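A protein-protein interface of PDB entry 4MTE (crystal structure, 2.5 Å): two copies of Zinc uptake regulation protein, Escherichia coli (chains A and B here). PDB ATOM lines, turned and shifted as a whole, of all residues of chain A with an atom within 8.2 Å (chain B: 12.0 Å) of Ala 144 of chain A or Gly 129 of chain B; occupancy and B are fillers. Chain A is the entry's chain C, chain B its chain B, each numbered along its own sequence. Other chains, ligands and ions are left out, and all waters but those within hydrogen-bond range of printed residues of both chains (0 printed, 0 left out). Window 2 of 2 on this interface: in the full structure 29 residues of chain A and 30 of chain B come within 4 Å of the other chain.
Printed residues of chain B within 4 Å of Ala 144 of chain A: Gly 129 (3.4 Å). Of the printed residues of chain A, Gly 129 of chain B touches Ala 144 and Val 147. No residue of chain B comes within 4 Å of Cys 143 of chain A. No residue of chain B comes within 4 Å of Cys 146 of chain A. Of the printed residues of chain B, Val 147 of chain A touches Gly 129 (3.9 Å). Of the printed residues of chain A, Met 128 of chain B touches Glu 112 (3.3 Å). Printed residues of chain A within 4 Å of Phe 130 of chain B: Gly 141 and Leu 142. Of the printed residues of chain A, Ala 131 of chain B touches Gly 141 and Leu 142. His 122 of chain B touches none of the printed residues of chain A. Cys 106 of chain A touches none of the printed residues of chain B. The nearest residue of chain B that does not touch Ala 144 of chain A is Phe 130 of chain B (4.5 Å).
Of the 14 printed residues of chain B, 4 touch a printed residue of chain A. Along chain B the printed residues that touch a printed residue of chain A span positions 128 to 131. Of the 15 printed residues of chain A, 5 touch a printed residue of chain B. Hydrophobic or aromatic side chains of chain A that line the printed part of chain B: Ala 144 and Val 147. Among the printed residues, 7 pairs touch across the chains.
No position is printed for both chains. Of the 7 pairs that touch across the chains among the printed residues, none has its exchanged pair printed and touching as well.
Among the printed residues, merely in contact across the chains: Glu 112 of chain A with Met 128 of chain B, Gly 141 of chain A with Phe 130 of chain B, Gly 141 of chain A with Ala 131 of chain B, Leu 142 of chain A with Phe 130 of chain B, Ala 144 of chain A with Gly 129 of chain B and Val 147 of chain A with Gly 129 of chain B.
The backbone carbonyl oxygen (O) of Leu 142 of chain A sits at hydrogen-bond distance from the backbone NH (N) of Ala 131 of chain B, at 2.9 Å.
The backbone carbonyl oxygen (O) of Ala 125 of chain B sits at hydrogen-bond distance from the backbone NH (N) of Phe 130 of chain B, at 3.1 Å.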
ATOM      1  N   CYS A 103       9.771  -9.092  -5.886  1.00  0.00           N
ATOM      2  CA  CYS A 103       9.125  -7.910  -6.441  1.00  0.00           C
ATOM      3  C   CYS A 103       7.977  -7.482  -5.530  1.00  0.00           C
ATOM      4  O   CYS A 103       7.065  -8.264  -5.261  1.00  0.00           O
ATOM      5  CB  CYS A 103       8.604  -8.182  -7.854  1.00  0.00           C
ATOM      6  SG  CYS A 103       8.085  -6.690  -8.731  1.00  0.00           S
ATOM      7  N   CYS A 106       4.570  -7.202  -8.252  1.00  0.00           N
ATOM      8  CA  CYS A 106       3.912  -8.342  -8.893  1.00  0.00           C
ATOM      9  C   CYS A 106       4.003  -9.617  -8.052  1.00  0.00           C
ATOM     10  O   CYS A 106       3.286 -10.587  -8.308  1.00  0.00           O
ATOM     11  CB  CYS A 106       4.474  -8.579 -10.303  1.00  0.00           C
ATOM     12  SG  CYS A 106       6.101  -9.368 -10.385  1.00  0.00           S
ATOM     13  N   ALA A 108       6.540 -11.618  -7.822  1.00  0.00           N
ATOM     14  CA  ALA A 108       7.418 -12.609  -8.428  1.00  0.00           C
ATOM     15  C   ALA A 108       8.664 -12.789  -7.572  1.00  0.00           C
ATOM     16  O   ALA A 108       9.225 -11.814  -7.068  1.00  0.00           O
ATOM     17  CB  ALA A 108       7.803 -12.193  -9.844  1.00  0.00           C
ATOM     18  N   GLU A 112      18.232 -17.162  -6.369  1.00  0.00           N
ATOM     19  CA  GLU A 112      19.584 -17.044  -6.896  1.00  0.00           C
ATOM     20  C   GLU A 112      20.570 -17.548  -5.855  1.00  0.00           C
ATOM     21  O   GLU A 112      20.192 -17.820  -4.715  1.00  0.00           O
ATOM     22  CB  GLU A 112      19.899 -15.587  -7.236  1.00  0.00           C
ATOM     23  CG  GLU A 112      18.941 -14.941  -8.226  1.00  0.00           C
ATOM     24  CD  GLU A 112      19.297 -15.227  -9.673  1.00  0.00           C
ATOM     25  OE1 GLU A 112      20.020 -16.211  -9.933  1.00  0.00           O
ATOM     26  OE2 GLU A 112      18.853 -14.459 -10.552  1.00  0.00           O
ATOM     27  N   GLY A 141      12.302  -5.390  -4.080  1.00  0.00           N
ATOM     28  CA  GLY A 141      12.376  -4.318  -5.053  1.00  0.00           C
ATOM     29  C   GLY A 141      11.402  -4.498  -6.196  1.00  0.00           C
ATOM     30  O   GLY A 141      10.259  -4.902  -5.988  1.00  0.00           O
ATOM     31  N   LEU A 142      11.861  -4.189  -7.404  1.00  0.00           N
ATOM     32  CA  LEU A 142      11.052  -4.335  -8.607  1.00  0.00           C
ATOM     33  C   LEU A 142      11.755  -5.249  -9.596  1.00  0.00           C
ATOM     34  O   LEU A 142      12.934  -5.058  -9.896  1.00  0.00           O
ATOM     35  CB  LEU A 142      10.816  -2.970  -9.259  1.00  0.00           C
ATOM     36  CG  LEU A 142      10.064  -1.930  -8.429  1.00  0.00           C
ATOM     37  CD1 LEU A 142      10.026  -0.604  -9.175  1.00  0.00           C
ATOM     38  CD2 LEU A 142       8.656  -2.413  -8.096  1.00  0.00           C
ATOM     39  N   CYS A 143      11.039  -6.249 -10.099  1.00  0.00           N
ATOM     40  CA  CYS A 143      11.565  -7.079 -11.172  1.00  0.00           C
ATOM     41  C   CYS A 143      11.647  -6.230 -12.438  1.00  0.00           C
ATOM     42  O   CYS A 143      10.958  -5.216 -12.553  1.00  0.00           O
ATOM     43  CB  CYS A 143      10.675  -8.302 -11.407  1.00  0.00           C
ATOM     44  SG  CYS A 143       9.066  -7.926 -12.143  1.00  0.00           S
ATOM     45  N   ALA A 144      12.490  -6.650 -13.376  1.00  0.00           N
ATOM     46  CA  ALA A 144      12.731  -5.920 -14.623  1.00  0.00           C
ATOM     47  C   ALA A 144      11.438  -5.513 -15.329  1.00  0.00           C
ATOM     48  O   ALA A 144      11.298  -4.379 -15.812  1.00  0.00           O
ATOM     49  CB  ALA A 144      13.574  -6.776 -15.551  1.00  0.00           C
ATOM     50  N   ALA A 145      10.499  -6.451 -15.390  1.00  0.00           N
ATOM     51  CA  ALA A 145       9.214  -6.217 -16.033  1.00  0.00           C
ATOM     52  C   ALA A 145       8.527  -5.001 -15.413  1.00  0.00           C
ATOM     53  O   ALA A 145       8.191  -4.045 -16.115  1.00  0.00           O
ATOM     54  CB  ALA A 145       8.330  -7.458 -15.916  1.00  0.00           C
ATOM     55  N   CYS A 146       8.347  -5.029 -14.094  1.00  0.00           N
ATOM     56  CA  CYS A 146       7.677  -3.942 -13.382  1.00  0.00           C
ATOM     57  C   CYS A 146       8.414  -2.617 -13.562  1.00  0.00           C
ATOM     58  O   CYS A 146       7.792  -1.555 -13.620  1.00  0.00           O
ATOM     59  CB  CYS A 146       7.548  -4.266 -11.892  1.00  0.00           C
ATOM     60  SG  CYS A 146       6.342  -5.554 -11.503  1.00  0.00           S
ATOM     61  N   VAL A 147       9.739  -2.683 -13.644  1.00  0.00           N
ATOM     62  CA  VAL A 147      10.541  -1.499 -13.930  1.00  0.00           C
ATOM     63  C   VAL A 147      10.122  -0.931 -15.280  1.00  0.00           C
ATOM     64  O   VAL A 147       9.821   0.258 -15.399  1.00  0.00           O
ATOM     65  CB  VAL A 147      12.058  -1.819 -13.957  1.00  0.00           C
ATOM     66  CG1 VAL A 147      12.868  -0.603 -14.415  1.00  0.00           C
ATOM     67  CG2 VAL A 147      12.532  -2.296 -12.593  1.00  0.00           C
ATOM     68  N   GLU A 148      10.104  -1.788 -16.298  1.00  0.00           N
ATOM     69  CA  GLU A 148       9.707  -1.359 -17.637  1.00  0.00           C
ATOM     70  C   GLU A 148       8.258  -0.874 -17.682  1.00  0.00           C
ATOM     71  O   GLU A 148       7.926   0.033 -18.444  1.00  0.00           O
ATOM     72  CB  GLU A 148       9.932  -2.484 -18.645  1.00  0.00           C
ATOM     73  CG  GLU A 148      11.402  -2.704 -18.948  1.00  0.00           C
ATOM     74  CD  GLU A 148      11.654  -3.908 -19.823  1.00  0.00           C
ATOM     75  OE1 GLU A 148      10.706  -4.375 -20.484  1.00  0.00           O
ATOM     76  OE2 GLU A 148      12.806  -4.392 -19.843  1.00  0.00           O
ATOM     77  N   VAL A 149       7.401  -1.476 -16.861  1.00  0.00           N
ATOM     78  CA  VAL A 149       6.031  -0.996 -16.715  1.00  0.00           C
ATOM     79  C   VAL A 149       6.037   0.425 -16.157  1.00  0.00           C
ATOM     80  O   VAL A 149       5.374   1.313 -16.689  1.00  0.00           O
ATOM     81  CB  VAL A 149       5.197  -1.913 -15.781  1.00  0.00           C
ATOM     82  CG1 VAL A 149       3.854  -1.267 -15.418  1.00  0.00           C
ATOM     83  CG2 VAL A 149       4.975  -3.273 -16.424  1.00  0.00           C
ATOM     84  N   GLU A 150       6.793   0.634 -15.083  1.00  0.00           N
ATOM     85  CA  GLU A 150       6.838   1.936 -14.423  1.00  0.00           C
ATOM     86  C   GLU A 150       7.595   2.982 -15.238  1.00  0.00           C
ATOM     87  O   GLU A 150       7.383   4.181 -15.056  1.00  0.00           O
ATOM     88  CB  GLU A 150       7.460   1.811 -13.030  1.00  0.00           C
ATOM     89  CG  GLU A 150       6.598   1.044 -12.036  1.00  0.00           C
ATOM     90  CD  GLU A 150       5.255   1.707 -11.793  1.00  0.00           C
ATOM     91  OE1 GLU A 150       5.179   2.951 -11.874  1.00  0.00           O
ATOM     92  OE2 GLU A 150       4.274   0.981 -11.527  1.00  0.00           O
ATOM     93  N   ALA A 151       8.480   2.530 -16.122  1.00  0.00           N
ATOM     94  CA  ALA A 151       9.199   3.430 -17.021  1.00  0.00           C
ATOM     95  C   ALA A 151       8.242   4.344 -17.788  1.00  0.00           C
ATOM     96  O   ALA A 151       8.566   5.497 -18.075  1.00  0.00           O
ATOM     97  CB  ALA A 151      10.058   2.629 -17.995  1.00  0.00           C
ATOM     98  N   ILE B 120      27.534  -7.024  -3.310  1.00  0.00           N
ATOM     99  CA  ILE B 120      27.271  -8.302  -3.974  1.00  0.00           C
ATOM    100  C   ILE B 120      25.823  -8.369  -4.452  1.00  0.00           C
ATOM    101  O   ILE B 120      25.553  -8.698  -5.609  1.00  0.00           O
ATOM    102  CB  ILE B 120      27.521  -9.526  -3.046  1.00  0.00           C
ATOM    103  CG1 ILE B 120      28.912  -9.484  -2.409  1.00  0.00           C
ATOM    104  CG2 ILE B 120      27.364 -10.832  -3.821  1.00  0.00           C
ATOM    105  CD1 ILE B 120      30.049  -9.185  -3.372  1.00  0.00           C
ATOM    106  N   MET B 121      24.899  -8.056  -3.551  1.00  0.00           N
ATOM    107  CA  MET B 121      23.472  -8.116  -3.848  1.00  0.00           C
ATOM    108  C   MET B 121      23.098  -7.127  -4.948  1.00  0.00           C
ATOM    109  O   MET B 121      22.272  -7.428  -5.807  1.00  0.00           O
ATOM    110  CB  MET B 121      22.661  -7.823  -2.586  1.00  0.00           C
ATOM    111  CG  MET B 121      22.809  -8.872  -1.498  1.00  0.00           C
ATOM    112  SD  MET B 121      22.093 -10.460  -1.950  1.00  0.00           S
ATOM    113  CE  MET B 121      20.342 -10.090  -1.906  1.00  0.00           C
ATOM    114  N   HIS B 122      23.707  -5.947  -4.911  1.00  0.00           N
ATOM    115  CA  HIS B 122      23.474  -4.932  -5.931  1.00  0.00           C
ATOM    116  C   HIS B 122      23.920  -5.450  -7.297  1.00  0.00           C
ATOM    117  O   HIS B 122      23.176  -5.381  -8.276  1.00  0.00           O
ATOM    118  CB  HIS B 122      24.239  -3.656  -5.583  1.00  0.00           C
ATOM    119  CG  HIS B 122      23.839  -2.468  -6.402  1.00  0.00           C
ATOM    120  ND1 HIS B 122      24.436  -2.156  -7.604  1.00  0.00           N
ATOM    121  CD2 HIS B 122      22.901  -1.515  -6.189  1.00  0.00           C
ATOM    122  CE1 HIS B 122      23.883  -1.063  -8.098  1.00  0.00           C
ATOM    123  NE2 HIS B 122      22.949  -0.654  -7.258  1.00  0.00           N
ATOM    124  N   THR B 123      25.143  -5.970  -7.347  1.00  0.00           N
ATOM    125  CA  THR B 123      25.696  -6.563  -8.564  1.00  0.00           C
ATOM    126  C   THR B 123      24.788  -7.668  -9.100  1.00  0.00           C
ATOM    127  O   THR B 123      24.426  -7.683 -10.282  1.00  0.00           O
ATOM    128  CB  THR B 123      27.107  -7.144  -8.289  1.00  0.00           C
ATOM    129  OG1 THR B 123      28.036  -6.070  -8.113  1.00  0.00           O
ATOM    130  CG2 THR B 123      27.588  -8.045  -9.431  1.00  0.00           C
ATOM    131  N   LEU B 124      24.429  -8.592  -8.217  1.00  0.00           N
ATOM    132  CA  LEU B 124      23.592  -9.730  -8.575  1.00  0.00           C
ATOM    133  C   LEU B 124      22.229  -9.267  -9.082  1.00  0.00           C
ATOM    134  O   LEU B 124      21.697  -9.809 -10.052  1.00  0.00           O
ATOM    135  CB  LEU B 124      23.414 -10.637  -7.359  1.00  0.00           C
ATOM    136  CG  LEU B 124      22.855 -12.038  -7.603  1.00  0.00           C
ATOM    137  CD1 LEU B 124      23.778 -12.858  -8.503  1.00  0.00           C
ATOM    138  CD2 LEU B 124      22.639 -12.735  -6.266  1.00  0.00           C
ATOM    139  N   ALA B 125      21.668  -8.261  -8.418  1.00  0.00           N
ATOM    140  CA  ALA B 125      20.396  -7.681  -8.830  1.00  0.00           C
ATOM    141  C   ALA B 125      20.565  -6.915 -10.137  1.00  0.00           C
ATOM    142  O   ALA B 125      19.632  -6.816 -10.932  1.00  0.00           O
ATOM    143  CB  ALA B 125      19.856  -6.755  -7.746  1.00  0.00           C
ATOM    144  N   ALA B 126      21.760  -6.370 -10.348  1.00  0.00           N
ATOM    145  CA  ALA B 126      22.056  -5.600 -11.554  1.00  0.00           C
ATOM    146  C   ALA B 126      22.299  -6.494 -12.767  1.00  0.00           C
ATOM    147  O   ALA B 126      22.059  -6.075 -13.898  1.00  0.00           O
ATOM    148  CB  ALA B 126      23.255  -4.689 -11.325  1.00  0.00           C
ATOM    149  N   LYS B 127      22.797  -7.709 -12.543  1.00  0.00           N
ATOM    150  CA  LYS B 127      22.904  -8.684 -13.632  1.00  0.00           C
ATOM    151  C   LYS B 127      21.538  -8.885 -14.283  1.00  0.00           C
ATOM    152  O   LYS B 127      21.386  -8.713 -15.492  1.00  0.00           O
ATOM    153  CB  LYS B 127      23.460 -10.021 -13.137  1.00  0.00           C
ATOM    154  CG  LYS B 127      24.895 -10.279 -13.567  1.00  0.00           C
ATOM    155  CD  LYS B 127      25.361 -11.667 -13.157  1.00  0.00           C
ATOM    156  CE  LYS B 127      24.973 -12.719 -14.188  1.00  0.00           C
ATOM    157  NZ  LYS B 127      25.905 -12.737 -15.352  1.00  0.00           N
ATOM    158  N   MET B 128      20.549  -9.248 -13.473  1.00  0.00           N
ATOM    159  CA  MET B 128      19.157  -9.227 -13.906  1.00  0.00           C
ATOM    160  C   MET B 128      18.701  -7.769 -13.918  1.00  0.00           C
ATOM    161  O   MET B 128      19.496  -6.874 -13.651  1.00  0.00           O
ATOM    162  CB  MET B 128      18.290 -10.075 -12.972  1.00  0.00           C
ATOM    163  CG  MET B 128      18.330  -9.650 -11.511  1.00  0.00           C
ATOM    164  SD  MET B 128      17.487 -10.802 -10.408  1.00  0.00           S
ATOM    165  CE  MET B 128      18.860 -11.393  -9.427  1.00  0.00           C
ATOM    166  N   GLY B 129      17.434  -7.517 -14.226  1.00  0.00           N
ATOM    167  CA  GLY B 129      16.951  -6.150 -14.313  1.00  0.00           C
ATOM    168  C   GLY B 129      16.315  -5.687 -13.017  1.00  0.00           C
ATOM    169  O   GLY B 129      15.492  -4.772 -13.009  1.00  0.00           O
ATOM    170  N   PHE B 130      16.712  -6.319 -11.916  1.00  0.00           N
ATOM    171  CA  PHE B 130      16.085  -6.073 -10.621  1.00  0.00           C
ATOM    172  C   PHE B 130      16.551  -4.750 -10.023  1.00  0.00           C
ATOM    173  O   PHE B 130      17.749  -4.475  -9.966  1.00  0.00           O
ATOM    174  CB  PHE B 130      16.392  -7.223  -9.655  1.00  0.00           C
ATOM    175  CG  PHE B 130      15.498  -7.254  -8.445  1.00  0.00           C
ATOM    176  CD1 PHE B 130      14.394  -8.090  -8.407  1.00  0.00           C
ATOM    177  CD2 PHE B 130      15.757  -6.448  -7.348  1.00  0.00           C
ATOM    178  CE1 PHE B 130      13.569  -8.121  -7.299  1.00  0.00           C
ATOM    179  CE2 PHE B 130      14.932  -6.479  -6.240  1.00  0.00           C
ATOM    180  CZ  PHE B 130      13.838  -7.316  -6.216  1.00  0.00           C
ATOM    181  N   ALA B 131      15.597  -3.935  -9.581  1.00  0.00           N
ATOM    182  CA  ALA B 131      15.904  -2.673  -8.912  1.00  0.00           C
ATOM    183  C   ALA B 131      15.823  -2.869  -7.404  1.00  0.00           C
ATOM    184  O   ALA B 131      14.737  -2.983  -6.841  1.00  0.00           O
ATOM    185  CB  ALA B 131      14.942  -1.580  -9.359  1.00  0.00           C
ATOM    186  N   LEU B 132      16.984  -2.900  -6.758  1.00  0.00           N
ATOM    187  CA  LEU B 132      17.075  -3.201  -5.336  1.00  0.00           C
ATOM    188  C   LEU B 132      16.624  -2.020  -4.478  1.00  0.00           C
ATOM    189  O   LEU B 132      16.992  -0.875  -4.743  1.00  0.00           O
ATOM    190  CB  LEU B 132      18.518  -3.570  -4.989  1.00  0.00           C
ATOM    191  CG  LEU B 132      18.751  -4.248  -3.642  1.00  0.00           C
ATOM    192  CD1 LEU B 132      18.168  -5.652  -3.643  1.00  0.00           C
ATOM    193  CD2 LEU B 132      20.239  -4.274  -3.327  1.00  0.00           C
ATOM    194  N   ARG B 133      15.825  -2.308  -3.453  1.00  0.00           N
ATOM    195  CA  ARG B 133      15.403  -1.297  -2.486  1.00  0.00           C
ATOM    196  C   ARG B 133      15.967  -1.610  -1.104  1.00  0.00           C
ATOM    197  O   ARG B 133      16.692  -0.800  -0.526  1.00  0.00           O
ATOM    198  CB  ARG B 133      13.877  -1.214  -2.422  1.00  0.00           C
ATOM    199  CG  ARG B 133      13.251  -0.419  -3.549  1.00  0.00           C
ATOM    200  CD  ARG B 133      11.740  -0.523  -3.509  1.00  0.00           C
ATOM    201  NE  ARG B 133      11.102   0.333  -4.503  1.00  0.00           N
ATOM    202  CZ  ARG B 133       9.792   0.369  -4.727  1.00  0.00           C
ATOM    203  NH1 ARG B 133       8.973  -0.410  -4.031  1.00  0.00           N
ATOM    204  NH2 ARG B 133       9.300   1.182  -5.652  1.00  0.00           N
